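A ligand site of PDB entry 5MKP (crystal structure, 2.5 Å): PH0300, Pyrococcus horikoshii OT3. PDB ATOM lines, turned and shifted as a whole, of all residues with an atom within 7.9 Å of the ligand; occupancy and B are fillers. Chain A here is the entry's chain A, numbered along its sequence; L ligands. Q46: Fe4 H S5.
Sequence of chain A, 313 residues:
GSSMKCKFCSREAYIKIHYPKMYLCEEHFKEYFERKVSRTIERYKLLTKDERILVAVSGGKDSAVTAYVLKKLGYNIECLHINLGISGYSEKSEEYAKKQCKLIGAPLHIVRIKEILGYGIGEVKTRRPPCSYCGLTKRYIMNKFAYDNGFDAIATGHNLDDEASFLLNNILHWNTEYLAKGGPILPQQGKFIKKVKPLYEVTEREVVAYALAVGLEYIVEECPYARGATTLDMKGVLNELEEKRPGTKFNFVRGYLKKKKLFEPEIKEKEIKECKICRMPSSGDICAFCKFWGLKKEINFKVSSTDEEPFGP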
ATOM      1  N   SER A  58      -6.987   4.213   5.212  1.00  0.00           N
ATOM      2  CA  SER A  58      -7.115   5.586   5.676  1.00  0.00           C
ATOM      3  C   SER A  58      -5.807   6.167   6.240  1.00  0.00           C
ATOM      4  O   SER A  58      -5.695   7.388   6.393  1.00  0.00           O
ATOM      5  CB  SER A  58      -8.186   5.646   6.766  1.00  0.00           C
ATOM      6  OG  SER A  58      -7.753   4.848   7.855  1.00  0.00           O
ATOM      7  N   ILE A  82      -8.170   7.297   0.221  1.00  0.00           N
ATOM      8  CA  ILE A  82      -8.948   8.475  -0.125  1.00  0.00           C
ATOM      9  C   ILE A  82      -8.426   9.654   0.681  1.00  0.00           C
ATOM     10  O   ILE A  82      -8.572   9.713   1.904  1.00  0.00           O
ATOM     11  CB  ILE A  82     -10.488   8.280  -0.007  1.00  0.00           C
ATOM     12  CG1 ILE A  82     -10.990   7.105  -0.897  1.00  0.00           C
ATOM     13  CG2 ILE A  82     -11.213   9.580  -0.363  1.00  0.00           C
ATOM     14  CD1 ILE A  82     -12.339   6.446  -0.488  1.00  0.00           C
ATOM     15  N   LEU A  84      -8.808  13.237   1.767  1.00  0.00           N
ATOM     16  CA  LEU A  84      -9.905  14.175   2.072  1.00  0.00           C
ATOM     17  C   LEU A  84      -9.573  15.665   1.876  1.00  0.00           C
ATOM     18  O   LEU A  84     -10.465  16.506   1.966  1.00  0.00           O
ATOM     19  CB  LEU A  84     -10.390  13.927   3.500  1.00  0.00           C
ATOM     20  CG  LEU A  84     -10.584  12.458   3.897  1.00  0.00           C
ATOM     21  CD1 LEU A  84     -10.748  12.319   5.381  1.00  0.00           C
ATOM     22  CD2 LEU A  84     -11.757  11.816   3.152  1.00  0.00           C
ATOM     23  N   ILE A  86      -7.854  17.774   3.770  1.00  0.00           N
ATOM     24  CA  ILE A  86      -7.912  18.513   5.024  1.00  0.00           C
ATOM     25  C   ILE A  86      -6.496  19.050   5.299  1.00  0.00           C
ATOM     26  O   ILE A  86      -5.607  18.262   5.651  1.00  0.00           O
ATOM     27  CB  ILE A  86      -8.460  17.621   6.185  1.00  0.00           C
ATOM     28  CG1 ILE A  86      -9.845  17.007   5.832  1.00  0.00           C
ATOM     29  CG2 ILE A  86      -8.521  18.417   7.509  1.00  0.00           C
ATOM     30  CD1 ILE A  86     -10.396  15.942   6.773  1.00  0.00           C
ATOM     31  N   TYR A  89      -3.649  17.621   7.759  1.00  0.00           N
ATOM     32  CA  TYR A  89      -4.071  16.268   8.164  1.00  0.00           C
ATOM     33  C   TYR A  89      -3.851  15.252   7.057  1.00  0.00           C
ATOM     34  O   TYR A  89      -3.191  14.235   7.247  1.00  0.00           O
ATOM     35  CB  TYR A  89      -5.560  16.253   8.536  1.00  0.00           C
ATOM     36  CG  TYR A  89      -5.831  16.062  10.012  1.00  0.00           C
ATOM     37  CD1 TYR A  89      -5.729  14.800  10.602  1.00  0.00           C
ATOM     38  CD2 TYR A  89      -6.217  17.129  10.810  1.00  0.00           C
ATOM     39  CE1 TYR A  89      -5.956  14.629  11.970  1.00  0.00           C
ATOM     40  CE2 TYR A  89      -6.480  16.963  12.168  1.00  0.00           C
ATOM     41  CZ  TYR A  89      -6.332  15.718  12.743  1.00  0.00           C
ATOM     42  OH  TYR A  89      -6.589  15.563  14.088  1.00  0.00           O
ATOM     43  N   ILE A 121     -12.825  18.152   2.733  1.00  0.00           N
ATOM     44  CA  ILE A 121     -13.827  17.918   3.774  1.00  0.00           C
ATOM     45  C   ILE A 121     -13.621  19.026   4.830  1.00  0.00           C
ATOM     46  O   ILE A 121     -12.532  19.128   5.404  1.00  0.00           O
ATOM     47  CB  ILE A 121     -13.698  16.482   4.354  1.00  0.00           C
ATOM     48  CG1 ILE A 121     -13.937  15.383   3.260  1.00  0.00           C
ATOM     49  CG2 ILE A 121     -14.585  16.267   5.600  1.00  0.00           C
ATOM     50  CD1 ILE A 121     -15.358  15.230   2.572  1.00  0.00           C
ATOM     51  N   GLY A 122     -14.630  19.871   5.003  1.00  0.00           N
ATOM     52  CA  GLY A 122     -14.615  21.005   5.909  1.00  0.00           C
ATOM     53  C   GLY A 122     -14.355  22.330   5.208  1.00  0.00           C
ATOM     54  O   GLY A 122     -13.993  23.316   5.856  1.00  0.00           O
ATOM     55  N   PRO A 129     -22.444  18.872   9.311  1.00  0.00           N
ATOM     56  CA  PRO A 129     -21.117  18.556   9.886  1.00  0.00           C
ATOM     57  C   PRO A 129     -20.214  17.804   8.907  1.00  0.00           C
ATOM     58  O   PRO A 129     -20.704  16.911   8.215  1.00  0.00           O
ATOM     59  CB  PRO A 129     -21.457  17.708  11.122  1.00  0.00           C
ATOM     60  CG  PRO A 129     -22.844  17.208  10.882  1.00  0.00           C
ATOM     61  CD  PRO A 129     -23.529  18.312  10.135  1.00  0.00           C
ATOM     62  N   PRO A 130     -18.909  18.190   8.826  1.00  0.00           N
ATOM     63  CA  PRO A 130     -17.989  17.535   7.881  1.00  0.00           C
ATOM     64  C   PRO A 130     -18.015  16.005   7.864  1.00  0.00           C
ATOM     65  O   PRO A 130     -17.948  15.445   6.775  1.00  0.00           O
ATOM     66  CB  PRO A 130     -16.625  18.070   8.309  1.00  0.00           C
ATOM     67  CG  PRO A 130     -16.920  19.417   8.826  1.00  0.00           C
ATOM     68  CD  PRO A 130     -18.208  19.260   9.571  1.00  0.00           C
ATOM     69  N   CYS A 131     -18.164  15.363   9.019  1.00  0.00           N
ATOM     70  CA  CYS A 131     -18.197  13.907   9.182  1.00  0.00           C
ATOM     71  C   CYS A 131     -19.331  13.193   8.439  1.00  0.00           C
ATOM     72  O   CYS A 131     -19.109  12.094   7.937  1.00  0.00           O
ATOM     73  CB  CYS A 131     -18.201  13.528  10.652  1.00  0.00           C
ATOM     74  SG  CYS A 131     -16.768  14.146  11.560  1.00  0.00           S
ATOM     75  N   SER A 132     -20.541  13.796   8.380  1.00  0.00           N
ATOM     76  CA  SER A 132     -21.668  13.160   7.683  1.00  0.00           C
ATOM     77  C   SER A 132     -21.443  13.058   6.169  1.00  0.00           C
ATOM     78  O   SER A 132     -21.569  11.949   5.613  1.00  0.00           O
ATOM     79  CB  SER A 132     -22.982  13.859   7.990  1.00  0.00           C
ATOM     80  OG  SER A 132     -22.919  15.219   7.590  1.00  0.00           O
ATOM     81  N   TYR A 133     -21.076  14.188   5.519  1.00  0.00           N
ATOM     82  CA  TYR A 133     -20.839  14.212   4.085  1.00  0.00           C
ATOM     83  C   TYR A 133     -19.500  13.546   3.705  1.00  0.00           C
ATOM     84  O   TYR A 133     -19.357  13.091   2.578  1.00  0.00           O
ATOM     85  CB  TYR A 133     -21.007  15.605   3.461  1.00  0.00           C
ATOM     86  CG  TYR A 133     -19.969  16.668   3.764  1.00  0.00           C
ATOM     87  CD1 TYR A 133     -18.824  16.792   2.980  1.00  0.00           C
ATOM     88  CD2 TYR A 133     -20.231  17.676   4.681  1.00  0.00           C
ATOM     89  CE1 TYR A 133     -17.930  17.846   3.162  1.00  0.00           C
ATOM     90  CE2 TYR A 133     -19.344  18.732   4.869  1.00  0.00           C
ATOM     91  CZ  TYR A 133     -18.192  18.803   4.123  1.00  0.00           C
ATOM     92  OH  TYR A 133     -17.324  19.854   4.324  1.00  0.00           O
ATOM     93  N   CYS A 134     -18.564  13.433   4.669  1.00  0.00           N
ATOM     94  CA  CYS A 134     -17.301  12.750   4.466  1.00  0.00           C
ATOM     95  C   CYS A 134     -17.543  11.246   4.361  1.00  0.00           C
ATOM     96  O   CYS A 134     -16.985  10.614   3.473  1.00  0.00           O
ATOM     97  CB  CYS A 134     -16.320  13.065   5.577  1.00  0.00           C
ATOM     98  SG  CYS A 134     -14.744  12.184   5.451  1.00  0.00           S
ATOM     99  N   GLY A 135     -18.369  10.708   5.261  1.00  0.00           N
ATOM    100  CA  GLY A 135     -18.756   9.291   5.275  1.00  0.00           C
ATOM    101  C   GLY A 135     -19.422   8.884   3.974  1.00  0.00           C
ATOM    102  O   GLY A 135     -19.095   7.827   3.408  1.00  0.00           O
ATOM    103  N   LEU A 136     -20.296   9.767   3.463  1.00  0.00           N
ATOM    104  CA  LEU A 136     -21.031   9.655   2.212  1.00  0.00           C
ATOM    105  C   LEU A 136     -20.034   9.613   1.053  1.00  0.00           C
ATOM    106  O   LEU A 136     -20.151   8.748   0.169  1.00  0.00           O
ATOM    107  CB  LEU A 136     -21.961  10.874   2.078  1.00  0.00           C
ATOM    108  CG  LEU A 136     -22.622  11.164   0.717  1.00  0.00           C
ATOM    109  CD1 LEU A 136     -23.896  10.375   0.560  1.00  0.00           C
ATOM    110  CD2 LEU A 136     -22.919  12.659   0.565  1.00  0.00           C
ATOM    111  N   LYS A 138     -16.561   9.057   1.134  1.00  0.00           N
ATOM    112  CA  LYS A 138     -15.669   7.890   1.242  1.00  0.00           C
ATOM    113  C   LYS A 138     -16.379   6.627   0.780  1.00  0.00           C
ATOM    114  O   LYS A 138     -15.887   5.981  -0.131  1.00  0.00           O
ATOM    115  CB  LYS A 138     -15.134   7.709   2.662  1.00  0.00           C
ATOM    116  CG  LYS A 138     -14.182   8.802   3.147  1.00  0.00           C
ATOM    117  CD  LYS A 138     -13.728   8.614   4.616  1.00  0.00           C
ATOM    118  CE  LYS A 138     -14.850   8.674   5.638  1.00  0.00           C
ATOM    119  NZ  LYS A 138     -14.383   8.439   7.032  1.00  0.00           N
ATOM    120  N   ARG A 139     -17.557   6.312   1.331  1.00  0.00           N
ATOM    121  CA  ARG A 139     -18.355   5.123   0.978  1.00  0.00           C
ATOM    122  C   ARG A 139     -18.693   5.021  -0.494  1.00  0.00           C
ATOM    123  O   ARG A 139     -18.713   3.910  -1.041  1.00  0.00           O
ATOM    124  CB  ARG A 139     -19.633   5.001   1.828  1.00  0.00           C
ATOM    125  CG  ARG A 139     -19.389   4.307   3.177  1.00  0.00           C
ATOM    126  CD  ARG A 139     -20.692   4.024   3.928  1.00  0.00           C
ATOM    127  NE  ARG A 139     -21.463   5.238   4.186  1.00  0.00           N
ATOM    128  CZ  ARG A 139     -21.336   6.002   5.274  1.00  0.00           C
ATOM    129  NH1 ARG A 139     -20.448   5.682   6.216  1.00  0.00           N
ATOM    130  NH2 ARG A 139     -22.079   7.090   5.420  1.00  0.00           N
ATOM    131  N   HIS A 158     -12.939  -2.199  10.247  1.00  0.00           N
ATOM    132  CA  HIS A 158     -13.771  -2.146  11.444  1.00  0.00           C
ATOM    133  C   HIS A 158     -13.599  -3.419  12.275  1.00  0.00           C
ATOM    134  O   HIS A 158     -13.617  -4.543  11.735  1.00  0.00           O
ATOM    135  CB  HIS A 158     -15.235  -1.896  11.099  1.00  0.00           C
ATOM    136  CG  HIS A 158     -15.465  -0.711  10.217  1.00  0.00           C
ATOM    137  ND1 HIS A 158     -15.362  -0.815   8.841  1.00  0.00           N
ATOM    138  CD2 HIS A 158     -15.832   0.555  10.532  1.00  0.00           C
ATOM    139  CE1 HIS A 158     -15.638   0.392   8.365  1.00  0.00           C
ATOM    140  NE2 HIS A 158     -15.932   1.241   9.338  1.00  0.00           N
ATOM    141  N   GLU A 221      -5.820  10.223  14.676  1.00  0.00           N
ATOM    142  CA  GLU A 221      -6.947  10.995  14.150  1.00  0.00           C
ATOM    143  C   GLU A 221      -6.815  11.203  12.657  1.00  0.00           C
ATOM    144  O   GLU A 221      -5.751  11.600  12.170  1.00  0.00           O
ATOM    145  CB  GLU A 221      -7.145  12.320  14.895  1.00  0.00           C
ATOM    146  CG  GLU A 221      -7.912  12.176  16.204  1.00  0.00           C
ATOM    147  CD  GLU A 221      -8.511  13.444  16.777  1.00  0.00           C
ATOM    148  OE1 GLU A 221      -7.863  14.510  16.696  1.00  0.00           O
ATOM    149  OE2 GLU A 221      -9.622  13.361  17.347  1.00  0.00           O
ATOM    150  N   GLU A 222      -7.890  10.902  11.918  1.00  0.00           N
ATOM    151  CA  GLU A 222      -7.968  11.071  10.466  1.00  0.00           C
ATOM    152  C   GLU A 222      -8.342  12.529  10.124  1.00  0.00           C
ATOM    153  O   GLU A 222      -7.985  13.016   9.055  1.00  0.00           O
ATOM    154  CB  GLU A 222      -9.004  10.076   9.863  1.00  0.00           C
ATOM    155  CG  GLU A 222      -8.520   8.633   9.738  1.00  0.00           C
ATOM    156  CD  GLU A 222      -8.588   7.698  10.945  1.00  0.00           C
ATOM    157  OE1 GLU A 222      -8.249   8.115  12.074  1.00  0.00           O
ATOM    158  OE2 GLU A 222      -8.919   6.501  10.732  1.00  0.00           O
ATOM    159  N   CYS A 223      -9.039  13.221  11.072  1.00  0.00           N
ATOM    160  CA  CYS A 223      -9.516  14.598  10.897  1.00  0.00           C
ATOM    161  C   CYS A 223      -9.638  15.361  12.241  1.00  0.00           C
ATOM    162  O   CYS A 223      -9.728  14.721  13.294  1.00  0.00           O
ATOM    163  CB  CYS A 223     -10.860  14.570  10.180  1.00  0.00           C
ATOM    164  SG  CYS A 223     -12.258  14.335  11.307  1.00  0.00           S
ATOM    165  N   PRO A 224      -9.785  16.716  12.229  1.00  0.00           N
ATOM    166  CA  PRO A 224     -10.010  17.426  13.493  1.00  0.00           C
ATOM    167  C   PRO A 224     -11.505  17.595  13.822  1.00  0.00           C
ATOM    168  O   PRO A 224     -11.858  18.298  14.759  1.00  0.00           O
ATOM    169  CB  PRO A 224      -9.352  18.789  13.232  1.00  0.00           C
ATOM    170  CG  PRO A 224      -9.534  19.018  11.742  1.00  0.00           C
ATOM    171  CD  PRO A 224      -9.743  17.665  11.079  1.00  0.00           C
ATOM    172  N   TYR A 225     -12.380  16.943  13.038  1.00  0.00           N
ATOM    173  CA  TYR A 225     -13.839  17.066  13.151  1.00  0.00           C
ATOM    174  C   TYR A 225     -14.529  15.887  13.859  1.00  0.00           C
ATOM    175  O   TYR A 225     -15.719  15.995  14.186  1.00  0.00           O
ATOM    176  CB  TYR A 225     -14.456  17.311  11.745  1.00  0.00           C
ATOM    177  CG  TYR A 225     -13.676  18.308  10.902  1.00  0.00           C
ATOM    178  CD1 TYR A 225     -13.424  19.597  11.376  1.00  0.00           C
ATOM    179  CD2 TYR A 225     -13.190  17.959   9.647  1.00  0.00           C
ATOM    180  CE1 TYR A 225     -12.694  20.504  10.611  1.00  0.00           C
ATOM    181  CE2 TYR A 225     -12.478  18.876   8.874  1.00  0.00           C
ATOM    182  CZ  TYR A 225     -12.235  20.145   9.359  1.00  0.00           C
ATOM    183  OH  TYR A 225     -11.519  21.056   8.608  1.00  0.00           O
ATOM    184  N   ALA A 226     -13.787  14.781  14.117  1.00  0.00           N
ATOM    185  CA  ALA A 226     -14.256  13.578  14.814  1.00  0.00           C
ATOM    186  C   ALA A 226     -14.557  13.894  16.275  1.00  0.00           C
ATOM    187  O   ALA A 226     -13.759  14.551  16.945  1.00  0.00           O
ATOM    188  CB  ALA A 226     -13.205  12.481  14.743  1.00  0.00           C
ATOM    189  N   ALA A 229     -17.226  12.998  18.740  1.00  0.00           N
ATOM    190  CA  ALA A 229     -18.440  12.259  18.380  1.00  0.00           C
ATOM    191  C   ALA A 229     -18.786  11.200  19.433  1.00  0.00           C
ATOM    192  O   ALA A 229     -17.974  10.931  20.325  1.00  0.00           O
ATOM    193  CB  ALA A 229     -18.275  11.614  17.004  1.00  0.00           C
ATOM    194  N   THR A 231     -19.080   7.812  19.268  1.00  0.00           N
ATOM    195  CA  THR A 231     -18.279   6.578  19.209  1.00  0.00           C
ATOM    196  C   THR A 231     -17.181   6.478  20.282  1.00  0.00           C
ATOM    197  O   THR A 231     -16.991   5.402  20.852  1.00  0.00           O
ATOM    198  CB  THR A 231     -17.693   6.341  17.804  1.00  0.00           C
ATOM    199  OG1 THR A 231     -17.055   7.529  17.321  1.00  0.00           O
ATOM    200  CG2 THR A 231     -18.749   5.843  16.801  1.00  0.00           C
HETATM  201  S4  Q46 L   1     -16.072  10.880   8.489  1.00  0.00           S
HETATM  202 FE1  Q46 L   1     -15.703  12.580  10.021  1.00  0.00          FE
HETATM  203 FE3  Q46 L   1     -14.211  10.288   9.694  1.00  0.00          FE
HETATM  204 FE2  Q46 L   1     -14.318  12.146   7.665  1.00  0.00          FE
HETATM  205  S3  Q46 L   1     -14.418  14.105   8.864  1.00  0.00           S
HETATM  206 FE4  Q46 L   1     -12.966  12.722   9.983  1.00  0.00          FE
HETATM  207  S2  Q46 L   1     -14.269  11.647  11.542  1.00  0.00           S
HETATM  208  S1  Q46 L   1     -12.446  11.088   8.452  1.00  0.00           S
HETATM  209  S5  Q46 L   1     -13.359   8.111  10.065  1.00  0.00           S
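S5 of the ligand sits close to NZ of Lys 138, 3.2 Å away. FE2 of the ligand is bound by SG of Cys 134, at 2.3 Å. The side-chain sulfur of Cys 131 binds an iron atom (FE1) of the ligand, at 2.4 Å. An iron atom (FE4) of the ligand is bound by the side-chain sulfur of Cys 223 (2.2 Å).
O of Leu 84 is in hydrogen-bond range of N of Ile 121. N of Tyr 225 lies close to SG of Cys 223 (3.1 Å). The side-chain sulfur of Cys 223 sits close to the backbone NH of Ala 226 (3.2 Å). The backbone carbonyl oxygen (O) of Tyr 225 lies close to the side-chain sulfur (SG) of Cys 131 (3.4 Å). O of Cys 223 is in hydrogen-bond range of OH of Tyr 89 (3.3 Å).
Leu 84 touches the ligand. CG2 of Ile 121 touches S3 of the ligand (3.9 Å). Gly 135 touches the ligand. CB of Glu 222 touches S1 of the ligand (3.9 Å). CB of Ala 226 touches S2 of the ligand, 3.5 Å away. Hydrophobic or aromatic side chains within 4 Å of the ligand: Leu 84, Ile 121 and Ala 226.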
